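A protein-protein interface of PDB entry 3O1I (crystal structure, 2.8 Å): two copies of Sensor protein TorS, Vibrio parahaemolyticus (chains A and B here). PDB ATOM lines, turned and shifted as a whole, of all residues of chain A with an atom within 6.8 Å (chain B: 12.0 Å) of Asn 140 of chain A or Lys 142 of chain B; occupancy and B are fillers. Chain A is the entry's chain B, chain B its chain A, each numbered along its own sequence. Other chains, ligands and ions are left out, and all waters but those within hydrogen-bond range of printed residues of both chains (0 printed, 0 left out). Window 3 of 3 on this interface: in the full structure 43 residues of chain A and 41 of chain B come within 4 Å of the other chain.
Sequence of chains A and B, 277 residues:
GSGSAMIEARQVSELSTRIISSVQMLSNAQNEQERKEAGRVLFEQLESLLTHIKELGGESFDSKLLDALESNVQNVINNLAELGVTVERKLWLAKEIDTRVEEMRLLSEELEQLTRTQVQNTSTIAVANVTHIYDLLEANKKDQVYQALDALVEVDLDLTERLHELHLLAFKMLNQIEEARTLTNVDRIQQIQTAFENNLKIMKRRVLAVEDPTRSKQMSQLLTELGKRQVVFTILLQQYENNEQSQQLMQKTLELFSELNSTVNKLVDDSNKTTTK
O of Glu 138 of chain B sits at hydrogen-bond distance from NZ of Lys 142 of chain A, at 3.3 Å. The side-chain amide oxygen (OD1) of Asn 140 of chain A is in hydrogen-bond range of the side-chain amino group (NZ) of Lys 142 of chain B.
The backbone carbonyl oxygen (O) of Leu 137 of chain A lies close to the side-chain amide oxygen (OD1) of Asn 140 of chain A. OD1 of Asn 140 of chain A sits close to O of Glu 138 of chain A (3.5 Å). The backbone carbonyl oxygen (O) of Glu 138 of chain B lies close to the side-chain amide nitrogen (ND2) of Asn 140 of chain B (3.4 Å).
CD1 of Leu 137 of chain A touches CD1 of Leu 137 of chain B (3.4 Å). Leu 137 of chain A touches Lys 142 of chain B. CG1 of Val 145 of chain B touches CD2 of Leu 137 of chain A, at 3.5 Å. Leu 137 of chain A touches Tyr 146 of chain B. CB of Glu 138 of chain A touches OH of Tyr 146 of chain B, at 3.5 Å. Lys 142 of chain A touches Leu 137 of chain B (CE to O, 3.8 Å). OD1 of Asn 140 of chain B touches NZ of Lys 142 of chain A (3.9 Å). Leu 137 of chain B touches Val 145 of chain A (CD2 to CG1, 3.3 Å).
Of chain B, only Lys 142 comes within 4 Å of Asn 140 of chain A. Lys 142 of chain B touches just these residues of chain A: Leu 137 and Asn 140. Of chain B, only Leu 137 (3.4 Å), Lys 142 (3.8 Å), Val 145 (3.5 Å) and Tyr 146 (3.2 Å) come within 4 Å of Leu 137 of chain A. No residue of chain B comes within 4 Å of Ala 139 of chain A. No residue of chain B comes within 4 Å of Lys 141 of chain A. Lys 142 of chain A touches just these residues of chain B: Leu 137 (3.8 Å), Glu 138 (3.3 Å) and Asn 140 (3.9 Å). Printed residues of chain A within 4 Å of Tyr 146 of chain B: Leu 137 and Glu 138. Printed residues of chain A within 4 Å of Leu 137 of chain B: Leu 137 (3.4 Å), Lys 142 (3.8 Å) and Val 145 (3.3 Å). His 132 of chain B touches none of the printed residues of chain A. Gln 144 of chain B touches none of the printed residues of chain A. The nearest printed residue of chain A that does not touch Asn 140 of chain B is Asn 140 of chain A (7.2 Å).
Of the 20 printed residues of chain B, 6 touch a printed residue of chain A. Hydrophobic or aromatic side chains of chain B that line the printed part of chain A: Leu 137, Val 145 and Tyr 146. Hydrophobic or aromatic side chains of chain A within 4 Å of the printed part of chain B: Leu 137 and Val 145. Among the printed residues, 10 pairs touch across the chains.
Leu 137 of chain A touches its own counterpart, Leu 137 of chain B. Leu 137 of chain A touches Lys 142 of chain B, and with the chains exchanged Lys 142 of chain A touches Leu 137 of chain B. Leu 137 of chain A touches Val 145 of chain B, and with the chains exchanged Val 145 of chain A touches Leu 137 of chain B. Asn 140 of chain A touches Lys 142 of chain B, and with the chains exchanged Lys 142 of chain A touches Asn 140 of chain B.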
ATOM      1  N   ASP A 135     -32.387 -30.209 -13.266  1.00  0.00           N
ATOM      2  CA  ASP A 135     -32.711 -29.467 -14.474  1.00  0.00           C
ATOM      3  C   ASP A 135     -32.565 -27.985 -14.204  1.00  0.00           C
ATOM      4  O   ASP A 135     -32.171 -27.227 -15.082  1.00  0.00           O
ATOM      5  CB  ASP A 135     -34.136 -29.770 -14.914  1.00  0.00           C
ATOM      6  CG  ASP A 135     -34.400 -31.251 -15.015  1.00  0.00           C
ATOM      7  OD1 ASP A 135     -33.529 -31.973 -15.549  1.00  0.00           O
ATOM      8  OD2 ASP A 135     -35.477 -31.695 -14.564  1.00  0.00           O
ATOM      9  N   LEU A 136     -32.887 -27.570 -12.986  1.00  0.00           N
ATOM     10  CA  LEU A 136     -32.763 -26.170 -12.634  1.00  0.00           C
ATOM     11  C   LEU A 136     -31.296 -25.778 -12.664  1.00  0.00           C
ATOM     12  O   LEU A 136     -30.938 -24.734 -13.206  1.00  0.00           O
ATOM     13  CB  LEU A 136     -33.320 -25.904 -11.234  1.00  0.00           C
ATOM     14  CG  LEU A 136     -34.795 -26.198 -10.970  1.00  0.00           C
ATOM     15  CD1 LEU A 136     -35.180 -25.634  -9.607  1.00  0.00           C
ATOM     16  CD2 LEU A 136     -35.651 -25.578 -12.062  1.00  0.00           C
ATOM     17  N   LEU A 137     -30.444 -26.623 -12.089  1.00  0.00           N
ATOM     18  CA  LEU A 137     -29.020 -26.332 -12.041  1.00  0.00           C
ATOM     19  C   LEU A 137     -28.383 -26.321 -13.433  1.00  0.00           C
ATOM     20  O   LEU A 137     -27.426 -25.584 -13.670  1.00  0.00           O
ATOM     21  CB  LEU A 137     -28.298 -27.328 -11.129  1.00  0.00           C
ATOM     22  CG  LEU A 137     -26.940 -26.822 -10.623  1.00  0.00           C
ATOM     23  CD1 LEU A 137     -27.145 -25.566  -9.796  1.00  0.00           C
ATOM     24  CD2 LEU A 137     -26.253 -27.878  -9.792  1.00  0.00           C
ATOM     25  N   GLU A 138     -28.907 -27.129 -14.352  1.00  0.00           N
ATOM     26  CA  GLU A 138     -28.382 -27.162 -15.716  1.00  0.00           C
ATOM     27  C   GLU A 138     -28.676 -25.833 -16.409  1.00  0.00           C
ATOM     28  O   GLU A 138     -27.778 -25.204 -16.964  1.00  0.00           O
ATOM     29  CB  GLU A 138     -29.012 -28.300 -16.518  1.00  0.00           C
ATOM     30  CG  GLU A 138     -28.606 -28.296 -17.985  1.00  0.00           C
ATOM     31  CD  GLU A 138     -29.226 -29.432 -18.778  1.00  0.00           C
ATOM     32  OE1 GLU A 138     -30.450 -29.603 -18.792  1.00  0.00           O
ATOM     33  OE2 GLU A 138     -28.382 -30.214 -19.450  1.00  0.00           O
ATOM     34  N   ALA A 139     -29.940 -25.413 -16.379  1.00  0.00           N
ATOM     35  CA  ALA A 139     -30.344 -24.148 -16.987  1.00  0.00           C
ATOM     36  C   ALA A 139     -29.872 -23.004 -16.100  1.00  0.00           C
ATOM     37  O   ALA A 139     -30.300 -21.869 -16.240  1.00  0.00           O
ATOM     38  CB  ALA A 139     -31.853 -24.095 -17.154  1.00  0.00           C
ATOM     39  N   ASN A 140     -28.987 -23.331 -15.173  1.00  0.00           N
ATOM     40  CA  ASN A 140     -28.418 -22.363 -14.256  1.00  0.00           C
ATOM     41  C   ASN A 140     -29.387 -21.373 -13.615  1.00  0.00           C
ATOM     42  O   ASN A 140     -28.992 -20.251 -13.299  1.00  0.00           O
ATOM     43  CB  ASN A 140     -27.300 -21.590 -14.955  1.00  0.00           C
ATOM     44  CG  ASN A 140     -26.215 -22.502 -15.507  1.00  0.00           C
ATOM     45  OD1 ASN A 140     -25.728 -23.405 -14.818  1.00  0.00           O
ATOM     46  ND2 ASN A 140     -25.820 -22.260 -16.753  1.00  0.00           N
ATOM     47  N   LYS A 141     -30.641 -21.784 -13.411  1.00  0.00           N
ATOM     48  CA  LYS A 141     -31.648 -20.922 -12.779  1.00  0.00           C
ATOM     49  C   LYS A 141     -31.375 -20.831 -11.276  1.00  0.00           C
ATOM     50  O   LYS A 141     -32.215 -21.218 -10.464  1.00  0.00           O
ATOM     51  CB  LYS A 141     -33.058 -21.487 -12.993  1.00  0.00           C
ATOM     52  CG  LYS A 141     -33.475 -21.644 -14.444  1.00  0.00           C
ATOM     53  CD  LYS A 141     -34.906 -22.151 -14.532  1.00  0.00           C
ATOM     54  CE  LYS A 141     -35.344 -22.356 -15.972  1.00  0.00           C
ATOM     55  NZ  LYS A 141     -36.742 -22.877 -16.057  1.00  0.00           N
ATOM     56  N   LYS A 142     -30.202 -20.307 -10.925  1.00  0.00           N
ATOM     57  CA  LYS A 142     -29.752 -20.173  -9.540  1.00  0.00           C
ATOM     58  C   LYS A 142     -30.815 -19.835  -8.490  1.00  0.00           C
ATOM     59  O   LYS A 142     -30.949 -20.536  -7.494  1.00  0.00           O
ATOM     60  CB  LYS A 142     -28.620 -19.145  -9.460  1.00  0.00           C
ATOM     61  CG  LYS A 142     -27.680 -19.374  -8.287  1.00  0.00           C
ATOM     62  CD  LYS A 142     -26.620 -18.295  -8.174  1.00  0.00           C
ATOM     63  CE  LYS A 142     -25.675 -18.592  -7.025  1.00  0.00           C
ATOM     64  NZ  LYS A 142     -24.742 -17.463  -6.737  1.00  0.00           N
ATOM     65  N   ASP A 143     -31.565 -18.763  -8.698  1.00  0.00           N
ATOM     66  CA  ASP A 143     -32.595 -18.373  -7.739  1.00  0.00           C
ATOM     67  C   ASP A 143     -33.568 -19.511  -7.432  1.00  0.00           C
ATOM     68  O   ASP A 143     -34.024 -19.665  -6.300  1.00  0.00           O
ATOM     69  CB  ASP A 143     -33.370 -17.171  -8.282  1.00  0.00           C
ATOM     70  CG  ASP A 143     -32.468 -15.983  -8.571  1.00  0.00           C
ATOM     71  OD1 ASP A 143     -31.850 -15.466  -7.614  1.00  0.00           O
ATOM     72  OD2 ASP A 143     -32.373 -15.573  -9.752  1.00  0.00           O
ATOM     73  N   VAL A 145     -32.962 -22.949  -7.893  1.00  0.00           N
ATOM     74  CA  VAL A 145     -32.233 -24.014  -7.213  1.00  0.00           C
ATOM     75  C   VAL A 145     -32.263 -23.819  -5.701  1.00  0.00           C
ATOM     76  O   VAL A 145     -32.467 -24.768  -4.953  1.00  0.00           O
ATOM     77  CB  VAL A 145     -30.763 -24.078  -7.677  1.00  0.00           C
ATOM     78  CG1 VAL A 145     -29.959 -24.973  -6.743  1.00  0.00           C
ATOM     79  CG2 VAL A 145     -30.690 -24.609  -9.108  1.00  0.00           C
ATOM     80  N   HIS B 132     -24.645 -27.039   2.956  1.00  0.00           N
ATOM     81  CA  HIS B 132     -23.361 -26.963   2.289  1.00  0.00           C
ATOM     82  C   HIS B 132     -23.554 -26.855   0.783  1.00  0.00           C
ATOM     83  O   HIS B 132     -22.681 -26.366   0.070  1.00  0.00           O
ATOM     84  CB  HIS B 132     -22.557 -28.208   2.610  1.00  0.00           C
ATOM     85  CG  HIS B 132     -21.184 -28.205   2.024  1.00  0.00           C
ATOM     86  ND1 HIS B 132     -20.142 -27.491   2.576  1.00  0.00           N
ATOM     87  CD2 HIS B 132     -20.675 -28.851   0.947  1.00  0.00           C
ATOM     88  CE1 HIS B 132     -19.048 -27.703   1.868  1.00  0.00           C
ATOM     89  NE2 HIS B 132     -19.344 -28.525   0.874  1.00  0.00           N
ATOM     90  N   ILE B 133     -24.688 -27.338   0.294  1.00  0.00           N
ATOM     91  CA  ILE B 133     -24.978 -27.259  -1.125  1.00  0.00           C
ATOM     92  C   ILE B 133     -25.122 -25.772  -1.427  1.00  0.00           C
ATOM     93  O   ILE B 133     -24.719 -25.300  -2.489  1.00  0.00           O
ATOM     94  CB  ILE B 133     -26.308 -27.951  -1.474  1.00  0.00           C
ATOM     95  CG1 ILE B 133     -26.367 -29.346  -0.850  1.00  0.00           C
ATOM     96  CG2 ILE B 133     -26.449 -28.048  -2.990  1.00  0.00           C
ATOM     97  CD1 ILE B 133     -25.546 -30.395  -1.569  1.00  0.00           C
ATOM     98  N   TYR B 134     -25.703 -25.045  -0.471  1.00  0.00           N
ATOM     99  CA  TYR B 134     -25.924 -23.601  -0.587  1.00  0.00           C
ATOM    100  C   TYR B 134     -24.627 -22.865  -0.905  1.00  0.00           C
ATOM    101  O   TYR B 134     -24.459 -22.325  -1.999  1.00  0.00           O
ATOM    102  CB  TYR B 134     -26.505 -23.033   0.720  1.00  0.00           C
ATOM    103  CG  TYR B 134     -27.961 -23.367   1.005  1.00  0.00           C
ATOM    104  CD1 TYR B 134     -28.505 -23.157   2.275  1.00  0.00           C
ATOM    105  CD2 TYR B 134     -28.799 -23.875   0.007  1.00  0.00           C
ATOM    106  CE1 TYR B 134     -29.844 -23.442   2.547  1.00  0.00           C
ATOM    107  CE2 TYR B 134     -30.141 -24.164   0.270  1.00  0.00           C
ATOM    108  CZ  TYR B 134     -30.655 -23.947   1.542  1.00  0.00           C
ATOM    109  OH  TYR B 134     -31.974 -24.245   1.811  1.00  0.00           O
ATOM    110  N   ASP B 135     -23.716 -22.842   0.064  1.00  0.00           N
ATOM    111  CA  ASP B 135     -22.435 -22.166  -0.098  1.00  0.00           C
ATOM    112  C   ASP B 135     -21.721 -22.655  -1.355  1.00  0.00           C
ATOM    113  O   ASP B 135     -21.086 -21.875  -2.067  1.00  0.00           O
ATOM    114  CB  ASP B 135     -21.553 -22.403   1.132  1.00  0.00           C
ATOM    115  CG  ASP B 135     -22.267 -22.069   2.439  1.00  0.00           C
ATOM    116  OD1 ASP B 135     -23.214 -21.250   2.412  1.00  0.00           O
ATOM    117  OD2 ASP B 135     -21.873 -22.617   3.493  1.00  0.00           O
ATOM    118  N   LEU B 136     -21.835 -23.951  -1.620  1.00  0.00           N
ATOM    119  CA  LEU B 136     -21.216 -24.562  -2.791  1.00  0.00           C
ATOM    120  C   LEU B 136     -21.853 -24.037  -4.082  1.00  0.00           C
ATOM    121  O   LEU B 136     -21.201 -23.958  -5.119  1.00  0.00           O
ATOM    122  CB  LEU B 136     -21.364 -26.088  -2.715  1.00  0.00           C
ATOM    123  CG  LEU B 136     -20.905 -26.927  -3.907  1.00  0.00           C
ATOM    124  CD1 LEU B 136     -19.411 -26.795  -4.082  1.00  0.00           C
ATOM    125  CD2 LEU B 136     -21.281 -28.374  -3.684  1.00  0.00           C
ATOM    126  N   LEU B 137     -23.127 -23.672  -4.011  1.00  0.00           N
ATOM    127  CA  LEU B 137     -23.846 -23.167  -5.175  1.00  0.00           C
ATOM    128  C   LEU B 137     -23.463 -21.735  -5.512  1.00  0.00           C
ATOM    129  O   LEU B 137     -23.181 -21.410  -6.665  1.00  0.00           O
ATOM    130  CB  LEU B 137     -25.353 -23.239  -4.928  1.00  0.00           C
ATOM    131  CG  LEU B 137     -26.269 -22.725  -6.038  1.00  0.00           C
ATOM    132  CD1 LEU B 137     -26.039 -23.514  -7.318  1.00  0.00           C
ATOM    133  CD2 LEU B 137     -27.703 -22.860  -5.590  1.00  0.00           C
ATOM    134  N   GLU B 138     -23.468 -20.879  -4.499  1.00  0.00           N
ATOM    135  CA  GLU B 138     -23.134 -19.473  -4.674  1.00  0.00           C
ATOM    136  C   GLU B 138     -21.785 -19.298  -5.373  1.00  0.00           C
ATOM    137  O   GLU B 138     -21.661 -18.492  -6.296  1.00  0.00           O
ATOM    138  CB  GLU B 138     -23.121 -18.785  -3.313  1.00  0.00           C
ATOM    139  CG  GLU B 138     -23.002 -17.288  -3.385  1.00  0.00           C
ATOM    140  CD  GLU B 138     -23.070 -16.643  -2.019  1.00  0.00           C
ATOM    141  OE1 GLU B 138     -22.227 -16.896  -1.156  1.00  0.00           O
ATOM    142  OE2 GLU B 138     -24.079 -15.803  -1.812  1.00  0.00           O
ATOM    143  N   ALA B 139     -20.783 -20.056  -4.936  1.00  0.00           N
ATOM    144  CA  ALA B 139     -19.450 -19.994  -5.527  1.00  0.00           C
ATOM    145  C   ALA B 139     -19.487 -20.488  -6.979  1.00  0.00           C
ATOM    146  O   ALA B 139     -18.467 -20.502  -7.670  1.00  0.00           O
ATOM    147  CB  ALA B 139     -18.474 -20.835  -4.707  1.00  0.00           C
ATOM    148  N   ASN B 140     -20.669 -20.905  -7.425  1.00  0.00           N
ATOM    149  CA  ASN B 140     -20.885 -21.384  -8.789  1.00  0.00           C
ATOM    150  C   ASN B 140     -20.156 -22.662  -9.209  1.00  0.00           C
ATOM    151  O   ASN B 140     -20.066 -22.951 -10.404  1.00  0.00           O
ATOM    152  CB  ASN B 140     -20.546 -20.276  -9.789  1.00  0.00           C
ATOM    153  CG  ASN B 140     -21.375 -19.030  -9.580  1.00  0.00           C
ATOM    154  OD1 ASN B 140     -22.601 -19.095  -9.501  1.00  0.00           O
ATOM    155  ND2 ASN B 140     -20.712 -17.884  -9.497  1.00  0.00           N
ATOM    156  N   LYS B 141     -19.642 -23.431  -8.252  1.00  0.00           N
ATOM    157  CA  LYS B 141     -18.946 -24.669  -8.599  1.00  0.00           C
ATOM    158  C   LYS B 141     -19.990 -25.739  -8.911  1.00  0.00           C
ATOM    159  O   LYS B 141     -19.966 -26.844  -8.380  1.00  0.00           O
ATOM    160  CB  LYS B 141     -18.020 -25.093  -7.451  1.00  0.00           C
ATOM    161  CG  LYS B 141     -17.036 -23.994  -7.070  1.00  0.00           C
ATOM    162  CD  LYS B 141     -15.882 -24.464  -6.206  1.00  0.00           C
ATOM    163  CE  LYS B 141     -14.876 -23.323  -6.024  1.00  0.00           C
ATOM    164  NZ  LYS B 141     -13.641 -23.715  -5.286  1.00  0.00           N
ATOM    165  N   LYS B 142     -20.906 -25.368  -9.798  1.00  0.00           N
ATOM    166  CA  LYS B 142     -22.008 -26.211 -10.238  1.00  0.00           C
ATOM    167  C   LYS B 142     -21.665 -27.679 -10.463  1.00  0.00           C
ATOM    168  O   LYS B 142     -22.508 -28.557 -10.261  1.00  0.00           O
ATOM    169  CB  LYS B 142     -22.613 -25.621 -11.517  1.00  0.00           C
ATOM    170  CG  LYS B 142     -23.124 -24.197 -11.325  1.00  0.00           C
ATOM    171  CD  LYS B 142     -23.690 -23.593 -12.597  1.00  0.00           C
ATOM    172  CE  LYS B 142     -24.029 -22.125 -12.369  1.00  0.00           C
ATOM    173  NZ  LYS B 142     -24.421 -21.417 -13.619  1.00  0.00           N
ATOM    174  N   ASP B 143     -20.436 -27.951 -10.884  1.00  0.00           N
ATOM    175  CA  ASP B 143     -20.024 -29.326 -11.126  1.00  0.00           C
ATOM    176  C   ASP B 143     -20.035 -30.120  -9.823  1.00  0.00           C
ATOM    177  O   ASP B 143     -20.428 -31.288  -9.794  1.00  0.00           O
ATOM    178  CB  ASP B 143     -18.628 -29.355 -11.748  1.00  0.00           C
ATOM    179  CG  ASP B 143     -18.186 -30.758 -12.110  1.00  0.00           C
ATOM    180  OD1 ASP B 143     -19.009 -31.512 -12.682  1.00  0.00           O
ATOM    181  OD2 ASP B 143     -17.016 -31.101 -11.834  1.00  0.00           O
ATOM    182  N   GLN B 144     -19.601 -29.474  -8.748  1.00  0.00           N
ATOM    183  CA  GLN B 144     -19.572 -30.108  -7.443  1.00  0.00           C
ATOM    184  C   GLN B 144     -20.981 -30.162  -6.873  1.00  0.00           C
ATOM    185  O   GLN B 144     -21.409 -31.204  -6.387  1.00  0.00           O
ATOM    186  CB  GLN B 144     -18.637 -29.344  -6.504  1.00  0.00           C
ATOM    187  CG  GLN B 144     -17.167 -29.518  -6.849  1.00  0.00           C
ATOM    188  CD  GLN B 144     -16.263 -28.523  -6.142  1.00  0.00           C
ATOM    189  OE1 GLN B 144     -16.201 -28.483  -4.913  1.00  0.00           O
ATOM    190  NE2 GLN B 144     -15.552 -27.712  -6.924  1.00  0.00           N
ATOM    191  N   VAL B 145     -21.704 -29.046  -6.941  1.00  0.00           N
ATOM    192  CA  VAL B 145     -23.074 -29.004  -6.438  1.00  0.00           C
ATOM    193  C   VAL B 145     -23.838 -30.198  -6.995  1.00  0.00           C
ATOM    194  O   VAL B 145     -24.738 -30.732  -6.347  1.00  0.00           O
ATOM    195  CB  VAL B 145     -23.804 -27.717  -6.860  1.00  0.00           C
ATOM    196  CG1 VAL B 145     -25.252 -27.767  -6.398  1.00  0.00           C
ATOM    197  CG2 VAL B 145     -23.116 -26.508  -6.262  1.00  0.00           C
ATOM    198  N   TYR B 146     -23.476 -30.604  -8.207  1.00  0.00           N
ATOM    199  CA  TYR B 146     -24.106 -31.754  -8.830  1.00  0.00           C
ATOM    200  C   TYR B 146     -23.799 -32.963  -7.964  1.00  0.00           C
ATOM    201  O   TYR B 146     -24.702 -33.632  -7.472  1.00  0.00           O
ATOM    202  CB  TYR B 146     -23.550 -31.987 -10.238  1.00  0.00           C
ATOM    203  CG  TYR B 146     -24.448 -31.497 -11.347  1.00  0.00           C
ATOM    204  CD1 TYR B 146     -24.809 -30.155 -11.437  1.00  0.00           C
ATOM    205  CD2 TYR B 146     -24.955 -32.378 -12.295  1.00  0.00           C
ATOM    206  CE1 TYR B 146     -25.662 -29.701 -12.444  1.00  0.00           C
ATOM    207  CE2 TYR B 146     -25.804 -31.935 -13.308  1.00  0.00           C
ATOM    208  CZ  TYR B 146     -26.158 -30.600 -13.374  1.00  0.00           C
ATOM    209  OH  TYR B 146     -27.026 -30.178 -14.355  1.00  0.00           O
ATOM    210  N   GLN B 147     -22.515 -33.235  -7.776  1.00  0.00           N
ATOM    211  CA  GLN B 147     -22.093 -34.367  -6.968  1.00  0.00           C
ATOM    212  C   GLN B 147     -22.758 -34.304  -5.599  1.00  0.00           C
ATOM    213  O   GLN B 147     -23.428 -35.245  -5.182  1.00  0.00           O
ATOM    214  CB  GLN B 147     -20.568 -34.371  -6.799  1.00  0.00           C
ATOM    215  CG  GLN B 147     -19.778 -34.389  -8.099  1.00  0.00           C
ATOM    216  CD  GLN B 147     -20.150 -35.553  -8.996  1.00  0.00           C
ATOM    217  OE1 GLN B 147     -19.977 -36.717  -8.629  1.00  0.00           O
ATOM    218  NE2 GLN B 147     -20.666 -35.243 -10.184  1.00  0.00           N
ATOM    219  N   ALA B 148     -22.579 -33.187  -4.905  1.00  0.00           N
ATOM    220  CA  ALA B 148     -23.151 -33.012  -3.576  1.00  0.00           C
ATOM    221  C   ALA B 148     -24.632 -33.354  -3.525  1.00  0.00           C
ATOM    222  O   ALA B 148     -25.173 -33.604  -2.446  1.00  0.00           O
ATOM    223  CB  ALA B 148     -22.932 -31.594  -3.094  1.00  0.00           C
ATOM    224  N   LEU B 149     -25.287 -33.349  -4.683  1.00  0.00           N
ATOM    225  CA  LEU B 149     -26.701 -33.693  -4.751  1.00  0.00           C
ATOM    226  C   LEU B 149     -26.842 -35.199  -4.873  1.00  0.00           C
ATOM    227  O   LEU B 149     -27.701 -35.797  -4.242  1.00  0.00           O
ATOM    228  CB  LEU B 149     -27.378 -33.031  -5.952  1.00  0.00           C
ATOM    229  CG  LEU B 149     -27.686 -31.537  -5.867  1.00  0.00           C
ATOM    230  CD1 LEU B 149     -28.447 -31.127  -7.113  1.00  0.00           C
ATOM    231  CD2 LEU B 149     -28.515 -31.238  -4.629  1.00  0.00           C
ATOM    232  N   ASP B 150     -25.992 -35.810  -5.690  1.00  0.00           N
ATOM    233  CA  ASP B 150     -26.024 -37.255  -5.891  1.00  0.00           C
ATOM    234  C   ASP B 150     -25.857 -38.022  -4.576  1.00  0.00           C
ATOM    235  O   ASP B 150     -26.525 -39.037  -4.346  1.00  0.00           O
ATOM    236  CB  ASP B 150     -24.922 -37.673  -6.864  1.00  0.00           C
ATOM    237  CG  ASP B 150     -25.168 -37.174  -8.266  1.00  0.00           C
ATOM    238  OD1 ASP B 150     -26.188 -37.582  -8.856  1.00  0.00           O
ATOM    239  OD2 ASP B 150     -24.353 -36.376  -8.778  1.00  0.00           O
ATOM    240  N   ALA B 151     -24.956 -37.544  -3.724  1.00  0.00           N
ATOM    241  CA  ALA B 151     -24.715 -38.190  -2.444  1.00  0.00           C
ATOM    242  C   ALA B 151     -25.964 -38.009  -1.586  1.00  0.00           C
ATOM    243  O   ALA B 151     -26.484 -38.969  -1.019  1.00  0.00           O
ATOM    244  CB  ALA B 151     -23.500 -37.566  -1.763  1.00  0.00           C
